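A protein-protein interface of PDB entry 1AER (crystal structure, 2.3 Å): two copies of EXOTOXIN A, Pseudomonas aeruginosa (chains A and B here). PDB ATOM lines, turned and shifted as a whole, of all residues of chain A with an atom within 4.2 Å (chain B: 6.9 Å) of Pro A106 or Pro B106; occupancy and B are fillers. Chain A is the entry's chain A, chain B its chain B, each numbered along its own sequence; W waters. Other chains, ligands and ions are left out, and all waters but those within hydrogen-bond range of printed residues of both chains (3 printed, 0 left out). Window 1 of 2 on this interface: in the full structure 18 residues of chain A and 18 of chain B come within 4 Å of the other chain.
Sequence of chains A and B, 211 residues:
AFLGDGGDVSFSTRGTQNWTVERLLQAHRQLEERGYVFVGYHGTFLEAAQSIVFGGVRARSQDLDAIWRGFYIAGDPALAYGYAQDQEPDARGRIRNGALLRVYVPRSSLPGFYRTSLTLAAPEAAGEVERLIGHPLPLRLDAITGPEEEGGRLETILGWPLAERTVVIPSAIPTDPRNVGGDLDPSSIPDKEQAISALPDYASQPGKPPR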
ATOM      1  N   GLY A  35     -30.945 -13.584 -21.409  1.00  0.00           N
ATOM      2  CA  GLY A  35     -29.520 -13.483 -21.732  1.00  0.00           C
ATOM      3  C   GLY A  35     -28.976 -12.437 -22.692  1.00  0.00           C
ATOM      4  O   GLY A  35     -27.866 -12.627 -23.162  1.00  0.00           O
ATOM      5  N   TYR A  36     -29.751 -11.408 -23.054  1.00  0.00           N
ATOM      6  CA  TYR A  36     -29.263 -10.379 -23.949  1.00  0.00           C
ATOM      7  C   TYR A  36     -28.652  -9.220 -23.185  1.00  0.00           C
ATOM      8  O   TYR A  36     -29.067  -8.912 -22.062  1.00  0.00           O
ATOM      9  CB  TYR A  36     -30.347  -9.869 -24.853  1.00  0.00           C
ATOM     10  CG  TYR A  36     -30.624 -10.815 -25.968  1.00  0.00           C
ATOM     11  CD1 TYR A  36     -31.289 -12.025 -25.723  1.00  0.00           C
ATOM     12  CD2 TYR A  36     -30.142 -10.576 -27.260  1.00  0.00           C
ATOM     13  CE1 TYR A  36     -31.452 -12.979 -26.723  1.00  0.00           C
ATOM     14  CE2 TYR A  36     -30.308 -11.530 -28.281  1.00  0.00           C
ATOM     15  CZ  TYR A  36     -30.961 -12.723 -27.993  1.00  0.00           C
ATOM     16  OH  TYR A  36     -31.150 -13.678 -28.956  1.00  0.00           O
ATOM     17  N   VAL A  37     -27.642  -8.602 -23.798  1.00  0.00           N
ATOM     18  CA  VAL A  37     -26.939  -7.466 -23.237  1.00  0.00           C
ATOM     19  C   VAL A  37     -26.978  -6.256 -24.225  1.00  0.00           C
ATOM     20  O   VAL A  37     -26.833  -6.434 -25.445  1.00  0.00           O
ATOM     21  CB  VAL A  37     -25.475  -7.871 -22.944  1.00  0.00           C
ATOM     22  CG1 VAL A  37     -24.754  -8.120 -24.221  1.00  0.00           C
ATOM     23  CG2 VAL A  37     -24.770  -6.796 -22.142  1.00  0.00           C
ATOM     24  N   VAL A 105     -27.440  -7.865 -27.935  1.00  0.00           N
ATOM     25  CA  VAL A 105     -26.821  -9.085 -28.458  1.00  0.00           C
ATOM     26  C   VAL A 105     -26.720 -10.118 -27.302  1.00  0.00           C
ATOM     27  O   VAL A 105     -26.865  -9.770 -26.126  1.00  0.00           O
ATOM     28  CB  VAL A 105     -25.361  -8.865 -29.116  1.00  0.00           C
ATOM     29  CG1 VAL A 105     -25.390  -7.855 -30.263  1.00  0.00           C
ATOM     30  CG2 VAL A 105     -24.317  -8.508 -28.050  1.00  0.00           C
ATOM     31  N   PRO A 106     -26.546 -11.418 -27.629  1.00  0.00           N
ATOM     32  CA  PRO A 106     -26.436 -12.392 -26.540  1.00  0.00           C
ATOM     33  C   PRO A 106     -25.209 -12.101 -25.662  1.00  0.00           C
ATOM     34  O   PRO A 106     -24.136 -11.752 -26.141  1.00  0.00           O
ATOM     35  CB  PRO A 106     -26.262 -13.705 -27.306  1.00  0.00           C
ATOM     36  CG  PRO A 106     -27.092 -13.500 -28.513  1.00  0.00           C
ATOM     37  CD  PRO A 106     -26.657 -12.112 -28.931  1.00  0.00           C
ATOM     38  N   ARG A 107     -25.329 -12.296 -24.373  1.00  0.00           N
ATOM     39  CA  ARG A 107     -24.176 -12.075 -23.542  1.00  0.00           C
ATOM     40  C   ARG A 107     -23.016 -12.994 -23.978  1.00  0.00           C
ATOM     41  O   ARG A 107     -21.852 -12.586 -23.952  1.00  0.00           O
ATOM     42  CB  ARG A 107     -24.563 -12.291 -22.082  1.00  0.00           C
ATOM     43  CG  ARG A 107     -23.530 -11.836 -21.085  1.00  0.00           C
ATOM     44  CD  ARG A 107     -24.060 -11.845 -19.666  1.00  0.00           C
ATOM     45  NE  ARG A 107     -23.345 -10.853 -18.873  1.00  0.00           N
ATOM     46  CZ  ARG A 107     -23.790  -9.615 -18.658  1.00  0.00           C
ATOM     47  NH1 ARG A 107     -24.962  -9.228 -19.153  1.00  0.00           N
ATOM     48  NH2 ARG A 107     -23.071  -8.768 -17.924  1.00  0.00           N
ATOM     49  N   SER A 108     -23.321 -14.195 -24.472  1.00  0.00           N
ATOM     50  CA  SER A 108     -22.273 -15.128 -24.889  1.00  0.00           C
ATOM     51  C   SER A 108     -21.499 -14.731 -26.145  1.00  0.00           C
ATOM     52  O   SER A 108     -20.457 -15.298 -26.448  1.00  0.00           O
ATOM     53  CB  SER A 108     -22.798 -16.570 -24.965  1.00  0.00           C
ATOM     54  OG  SER A 108     -24.019 -16.677 -25.653  1.00  0.00           O
ATOM     55  N   SER A 109     -21.960 -13.698 -26.824  1.00  0.00           N
ATOM     56  CA  SER A 109     -21.262 -13.201 -28.001  1.00  0.00           C
ATOM     57  C   SER A 109     -20.171 -12.191 -27.644  1.00  0.00           C
ATOM     58  O   SER A 109     -19.298 -11.934 -28.461  1.00  0.00           O
ATOM     59  CB  SER A 109     -22.242 -12.523 -28.944  1.00  0.00           C
ATOM     60  OG  SER A 109     -23.243 -13.447 -29.368  1.00  0.00           O
ATOM     61  N   LEU A 110     -20.207 -11.632 -26.425  1.00  0.00           N
ATOM     62  CA  LEU A 110     -19.230 -10.628 -25.993  1.00  0.00           C
ATOM     63  C   LEU A 110     -17.746 -10.920 -26.236  1.00  0.00           C
ATOM     64  O   LEU A 110     -16.944 -10.019 -26.332  1.00  0.00           O
ATOM     65  CB  LEU A 110     -19.526 -10.160 -24.576  1.00  0.00           C
ATOM     66  CG  LEU A 110     -20.819  -9.325 -24.503  1.00  0.00           C
ATOM     67  CD1 LEU A 110     -21.070  -8.986 -23.077  1.00  0.00           C
ATOM     68  CD2 LEU A 110     -20.723  -8.040 -25.288  1.00  0.00           C
ATOM     69  N   ARG B  34     -17.421 -18.529 -30.434  1.00  0.00           N
ATOM     70  CA  ARG B  34     -18.267 -17.375 -30.400  1.00  0.00           C
ATOM     71  C   ARG B  34     -19.508 -17.565 -29.535  1.00  0.00           C
ATOM     72  O   ARG B  34     -20.479 -16.825 -29.667  1.00  0.00           O
ATOM     73  CB  ARG B  34     -18.627 -17.001 -31.800  1.00  0.00           C
ATOM     74  CG  ARG B  34     -17.436 -16.409 -32.503  1.00  0.00           C
ATOM     75  CD  ARG B  34     -16.935 -15.182 -31.730  1.00  0.00           C
ATOM     76  NE  ARG B  34     -15.931 -14.487 -32.525  1.00  0.00           N
ATOM     77  CZ  ARG B  34     -14.612 -14.615 -32.381  1.00  0.00           C
ATOM     78  NH1 ARG B  34     -14.128 -15.302 -31.367  1.00  0.00           N
ATOM     79  NH2 ARG B  34     -13.781 -13.954 -33.188  1.00  0.00           N
ATOM     80  N   GLY B  35     -19.461 -18.568 -28.656  1.00  0.00           N
ATOM     81  CA  GLY B  35     -20.531 -18.875 -27.699  1.00  0.00           C
ATOM     82  C   GLY B  35     -21.805 -19.592 -28.093  1.00  0.00           C
ATOM     83  O   GLY B  35     -22.785 -19.530 -27.352  1.00  0.00           O
ATOM     84  N   TYR B  36     -21.814 -20.225 -29.260  1.00  0.00           N
ATOM     85  CA  TYR B  36     -22.982 -20.952 -29.751  1.00  0.00           C
ATOM     86  C   TYR B  36     -22.907 -22.381 -29.297  1.00  0.00           C
ATOM     87  O   TYR B  36     -21.814 -22.937 -29.150  1.00  0.00           O
ATOM     88  CB  TYR B  36     -23.089 -20.872 -31.286  1.00  0.00           C
ATOM     89  CG  TYR B  36     -23.780 -19.598 -31.751  1.00  0.00           C
ATOM     90  CD1 TYR B  36     -23.086 -18.387 -31.872  1.00  0.00           C
ATOM     91  CD2 TYR B  36     -25.148 -19.578 -31.976  1.00  0.00           C
ATOM     92  CE1 TYR B  36     -23.755 -17.189 -32.190  1.00  0.00           C
ATOM     93  CE2 TYR B  36     -25.821 -18.388 -32.298  1.00  0.00           C
ATOM     94  CZ  TYR B  36     -25.125 -17.203 -32.399  1.00  0.00           C
ATOM     95  OH  TYR B  36     -25.836 -16.052 -32.713  1.00  0.00           O
ATOM     96  N   VAL B  37     -24.072 -22.958 -29.018  1.00  0.00           N
ATOM     97  CA  VAL B  37     -24.188 -24.340 -28.558  1.00  0.00           C
ATOM     98  C   VAL B  37     -25.183 -25.162 -29.417  1.00  0.00           C
ATOM     99  O   VAL B  37     -26.177 -24.635 -29.917  1.00  0.00           O
ATOM    100  CB  VAL B  37     -24.606 -24.435 -27.032  1.00  0.00           C
ATOM    101  CG1 VAL B  37     -23.530 -23.863 -26.141  1.00  0.00           C
ATOM    102  CG2 VAL B  37     -25.916 -23.683 -26.754  1.00  0.00           C
ATOM    103  N   TYR B 104     -27.732 -24.558 -33.759  1.00  0.00           N
ATOM    104  CA  TYR B 104     -27.028 -23.954 -32.614  1.00  0.00           C
ATOM    105  C   TYR B 104     -27.687 -22.681 -32.081  1.00  0.00           C
ATOM    106  O   TYR B 104     -28.214 -21.883 -32.850  1.00  0.00           O
ATOM    107  CB  TYR B 104     -25.585 -23.577 -33.021  1.00  0.00           C
ATOM    108  CG  TYR B 104     -24.658 -24.738 -33.334  1.00  0.00           C
ATOM    109  CD1 TYR B 104     -24.846 -25.513 -34.477  1.00  0.00           C
ATOM    110  CD2 TYR B 104     -23.603 -25.061 -32.481  1.00  0.00           C
ATOM    111  CE1 TYR B 104     -24.012 -26.585 -34.761  1.00  0.00           C
ATOM    112  CE2 TYR B 104     -22.771 -26.107 -32.744  1.00  0.00           C
ATOM    113  CZ  TYR B 104     -22.979 -26.872 -33.891  1.00  0.00           C
ATOM    114  OH  TYR B 104     -22.144 -27.911 -34.188  1.00  0.00           O
ATOM    115  N   VAL B 105     -27.611 -22.470 -30.776  1.00  0.00           N
ATOM    116  CA  VAL B 105     -28.149 -21.253 -30.161  1.00  0.00           C
ATOM    117  C   VAL B 105     -27.068 -20.746 -29.225  1.00  0.00           C
ATOM    118  O   VAL B 105     -26.176 -21.496 -28.883  1.00  0.00           O
ATOM    119  CB  VAL B 105     -29.372 -21.538 -29.263  1.00  0.00           C
ATOM    120  CG1 VAL B 105     -30.583 -21.973 -30.115  1.00  0.00           C
ATOM    121  CG2 VAL B 105     -28.997 -22.569 -28.173  1.00  0.00           C
ATOM    122  N   PRO B 106     -27.107 -19.456 -28.848  1.00  0.00           N
ATOM    123  CA  PRO B 106     -26.170 -18.791 -27.946  1.00  0.00           C
ATOM    124  C   PRO B 106     -26.241 -19.504 -26.620  1.00  0.00           C
ATOM    125  O   PRO B 106     -27.317 -19.745 -26.128  1.00  0.00           O
ATOM    126  CB  PRO B 106     -26.814 -17.445 -27.756  1.00  0.00           C
ATOM    127  CG  PRO B 106     -27.440 -17.206 -28.995  1.00  0.00           C
ATOM    128  CD  PRO B 106     -28.072 -18.479 -29.359  1.00  0.00           C
ATOM    129  N   ARG B 107     -25.111 -19.718 -25.972  1.00  0.00           N
ATOM    130  CA  ARG B 107     -25.093 -20.415 -24.709  1.00  0.00           C
ATOM    131  C   ARG B 107     -25.899 -19.678 -23.670  1.00  0.00           C
ATOM    132  O   ARG B 107     -26.379 -20.276 -22.706  1.00  0.00           O
ATOM    133  CB  ARG B 107     -23.652 -20.553 -24.249  1.00  0.00           C
ATOM    134  CG  ARG B 107     -23.491 -21.305 -22.936  1.00  0.00           C
ATOM    135  CD  ARG B 107     -22.131 -21.010 -22.305  1.00  0.00           C
ATOM    136  NE  ARG B 107     -21.895 -19.553 -22.190  1.00  0.00           N
ATOM    137  CZ  ARG B 107     -22.215 -18.777 -21.142  1.00  0.00           C
ATOM    138  NH1 ARG B 107     -22.809 -19.279 -20.054  1.00  0.00           N
ATOM    139  NH2 ARG B 107     -21.941 -17.473 -21.187  1.00  0.00           N
ATOM    140  N   SER B 108     -26.069 -18.373 -23.869  1.00  0.00           N
ATOM    141  CA  SER B 108     -26.794 -17.548 -22.908  1.00  0.00           C
ATOM    142  C   SER B 108     -28.301 -17.630 -23.004  1.00  0.00           C
ATOM    143  O   SER B 108     -29.017 -17.159 -22.105  1.00  0.00           O
ATOM    144  CB  SER B 108     -26.297 -16.080 -22.923  1.00  0.00           C
ATOM    145  OG  SER B 108     -26.308 -15.553 -24.219  1.00  0.00           O
ATOM    146  N   SER B 109     -28.793 -18.260 -24.065  1.00  0.00           N
ATOM    147  CA  SER B 109     -30.227 -18.400 -24.204  1.00  0.00           C
ATOM    148  C   SER B 109     -30.692 -19.642 -23.458  1.00  0.00           C
ATOM    149  O   SER B 109     -31.880 -19.764 -23.171  1.00  0.00           O
ATOM    150  CB  SER B 109     -30.638 -18.483 -25.667  1.00  0.00           C
ATOM    151  OG  SER B 109     -30.293 -19.749 -26.176  1.00  0.00           O
ATOM    152  N   LEU B 110     -29.760 -20.504 -23.051  1.00  0.00           N
ATOM    153  CA  LEU B 110     -30.126 -21.728 -22.339  1.00  0.00           C
ATOM    154  C   LEU B 110     -31.097 -21.644 -21.127  1.00  0.00           C
ATOM    155  O   LEU B 110     -31.805 -22.600 -20.838  1.00  0.00           O
ATOM    156  CB  LEU B 110     -28.899 -22.593 -22.059  1.00  0.00           C
ATOM    157  CG  LEU B 110     -28.251 -23.020 -23.384  1.00  0.00           C
ATOM    158  CD1 LEU B 110     -27.013 -23.790 -23.098  1.00  0.00           C
ATOM    159  CD2 LEU B 110     -29.153 -23.849 -24.233  1.00  0.00           C
ATOM    160  N   PRO B 111     -31.107 -20.542 -20.371  1.00  0.00           N
ATOM    161  CA  PRO B 111     -32.073 -20.536 -19.264  1.00  0.00           C
ATOM    162  C   PRO B 111     -33.550 -20.343 -19.708  1.00  0.00           C
ATOM    163  O   PRO B 111     -34.462 -20.336 -18.892  1.00  0.00           O
ATOM    164  CB  PRO B 111     -31.588 -19.371 -18.413  1.00  0.00           C
ATOM    165  CG  PRO B 111     -30.890 -18.484 -19.392  1.00  0.00           C
ATOM    166  CD  PRO B 111     -30.082 -19.510 -20.147  1.00  0.00           C
ATOM    167  N   PHE B 113     -34.796 -22.403 -21.892  1.00  0.00           N
ATOM    168  CA  PHE B 113     -35.088 -23.758 -22.402  1.00  0.00           C
ATOM    169  C   PHE B 113     -35.732 -24.580 -21.305  1.00  0.00           C
ATOM    170  O   PHE B 113     -35.093 -24.873 -20.300  1.00  0.00           O
ATOM    171  CB  PHE B 113     -33.810 -24.476 -22.782  1.00  0.00           C
ATOM    172  CG  PHE B 113     -33.361 -24.212 -24.155  1.00  0.00           C
ATOM    173  CD1 PHE B 113     -32.982 -22.949 -24.538  1.00  0.00           C
ATOM    174  CD2 PHE B 113     -33.331 -25.235 -25.088  1.00  0.00           C
ATOM    175  CE1 PHE B 113     -32.584 -22.696 -25.827  1.00  0.00           C
ATOM    176  CE2 PHE B 113     -32.924 -24.988 -26.404  1.00  0.00           C
ATOM    177  CZ  PHE B 113     -32.553 -23.710 -26.767  1.00  0.00           C
ATOM    178  N   LEU B 162     -36.449 -17.065 -31.340  1.00  0.00           N
ATOM    179  CA  LEU B 162     -35.195 -17.774 -31.038  1.00  0.00           C
ATOM    180  C   LEU B 162     -34.763 -18.548 -32.279  1.00  0.00           C
ATOM    181  O   LEU B 162     -33.583 -18.545 -32.661  1.00  0.00           O
ATOM    182  CB  LEU B 162     -35.402 -18.744 -29.875  1.00  0.00           C
ATOM    183  CG  LEU B 162     -34.131 -19.516 -29.508  1.00  0.00           C
ATOM    184  CD1 LEU B 162     -32.977 -18.602 -29.091  1.00  0.00           C
ATOM    185  CD2 LEU B 162     -34.336 -20.485 -28.342  1.00  0.00           C
ATOM    186  N   ARG B 165     -32.734 -16.687 -34.898  1.00  0.00           N
ATOM    187  CA  ARG B 165     -31.444 -16.179 -34.515  1.00  0.00           C
ATOM    188  C   ARG B 165     -30.447 -17.319 -34.268  1.00  0.00           C
ATOM    189  O   ARG B 165     -29.412 -17.118 -33.641  1.00  0.00           O
ATOM    190  CB  ARG B 165     -31.596 -15.336 -33.261  1.00  0.00           C
ATOM    191  CG  ARG B 165     -32.366 -14.089 -33.546  1.00  0.00           C
ATOM    192  CD  ARG B 165     -32.650 -13.245 -32.316  1.00  0.00           C
ATOM    193  NE  ARG B 165     -33.080 -11.924 -32.755  1.00  0.00           N
ATOM    194  CZ  ARG B 165     -34.296 -11.631 -33.160  1.00  0.00           C
ATOM    195  NH1 ARG B 165     -35.256 -12.538 -33.102  1.00  0.00           N
ATOM    196  NH2 ARG B 165     -34.556 -10.405 -33.566  1.00  0.00           N
ATOM    197  N   THR B 166     -30.763 -18.514 -34.740  1.00  0.00           N
ATOM    198  CA  THR B 166     -29.880 -19.646 -34.551  1.00  0.00           C
ATOM    199  C   THR B 166     -28.866 -19.678 -35.699  1.00  0.00           C
ATOM    200  O   THR B 166     -29.029 -18.950 -36.668  1.00  0.00           O
ATOM    201  CB  THR B 166     -30.697 -20.930 -34.674  1.00  0.00           C
ATOM    202  OG1 THR B 166     -31.392 -20.900 -35.929  1.00  0.00           O
ATOM    203  CG2 THR B 166     -31.692 -21.056 -33.537  1.00  0.00           C
ATOM    204  N   VAL B 167     -27.819 -20.503 -35.582  1.00  0.00           N
ATOM    205  CA  VAL B 167     -26.833 -20.725 -36.672  1.00  0.00           C
ATOM    206  C   VAL B 167     -27.032 -22.223 -37.037  1.00  0.00           C
ATOM    207  O   VAL B 167     -26.945 -23.100 -36.180  1.00  0.00           O
ATOM    208  CB  VAL B 167     -25.331 -20.478 -36.257  1.00  0.00           C
ATOM    209  CG1 VAL B 167     -24.422 -20.927 -37.393  1.00  0.00           C
ATOM    210  CG2 VAL B 167     -25.057 -18.995 -35.898  1.00  0.00           C
HETATM  211  O   HOH W   1     -23.204 -16.510 -27.964  1.00  0.00           O
HETATM  212  O   HOH W   2     -28.927 -14.705 -25.075  1.00  0.00           O
HETATM  213  O   HOH W   3     -21.610 -14.942 -30.989  1.00  0.00           O
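OG of Ser A108 is in hydrogen-bond range of N of Arg B107. O of Gly A35 sits at hydrogen-bond distance from OG of Ser B108, 3.5 Å away. The backbone NH of Arg A107 sits at hydrogen-bond distance from the side-chain hydroxyl of Ser B108. The side-chain hydroxyl (OG) of Ser B108 lies within hydrogen-bond range of the side-chain hydroxyl (OG) of Ser A108.
The side-chain hydroxyl (OG) of Ser B109 sits at hydrogen-bond distance from the backbone carbonyl oxygen (O) of Pro B106 (3.0 Å). The backbone NH of Arg A107 lies within hydrogen-bond range of the backbone carbonyl oxygen of Gly A35, at 2.8 Å. The backbone NH (N) of Arg B107 lies within hydrogen-bond range of the backbone carbonyl oxygen (O) of Gly B35 (2.7 Å).
Among the printed residues, merely in contact across the chains: Tyr A36 with Arg B165 (3.7 Å), Pro A106 with Pro B106 (3.8 Å), Pro A106 with Ser B108 (3.6 Å), Ser A108 with Arg B34 (3.6 Å), Ser A108 with Gly B35 (3.5 Å) and Ser A108 with Pro B106 (3.6 Å).
Printed residues of chain B within 4 Å of Gly A35: Ser B108 (3.5 Å). Val A37 touches none of the printed residues of chain B. Of chain B, only Pro B106 (3.8 Å) and Ser B108 (3.6 Å) come within 4 Å of Pro A106. Of the printed residues of chain A, Ser B108 touches Gly A35, Pro A106, Arg A107 and Ser A108. Leu B110 touches none of the printed residues of chain A. The nearest printed residue of chain A that does not touch Pro B106 is Tyr A36 (5.1 Å). The nearest printed residue of chain A that does not touch Ser B108 is Ser A109 (5.4 Å).
Of the 17 printed residues of chain B, 6 touch a printed residue of chain A. Printed residues of chain B that touch a printed residue of chain A: Arg B34, Gly B35, Pro B106, Arg B107, Ser B108 and Arg B165. Hydrophobic or aromatic side chains of chain B that line the printed part of chain A: Pro B106. Of the 9 printed residues of chain A, 5 touch a printed residue of chain B. Hydrophobic or aromatic side chains of chain A within 4 Å of the printed part of chain B: Tyr A36 and Pro A106. Among the printed residues, no Asp or Glu carboxylate lies within 4 Å of a Lys or Arg side-chain nitrogen of the other chain.
Pro B106 touches its own counterpart, Pro A106. Pro A106 touches Ser B108, and with the chains exchanged Ser A108 touches Pro B106. Arg A107 touches Ser B108, and with the chains exchanged Ser A108 touches Arg B107. Ser A108 touches its own counterpart, Ser B108. 9 positions are printed for both chains.
Water W1 lies within hydrogen-bond range of the side-chain hydroxyl of Ser A108, the backbone carbonyl oxygen of Gly B35, the backbone carbonyl oxygen of Arg B34 and the backbone NH of Ser A109. Water W3 lies within hydrogen-bond range of O of Arg B34 and OG of Ser A109. Water W2 bridges OG of Ser B108 (2.9 Å) and O of Gly A35 (3.0 Å).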
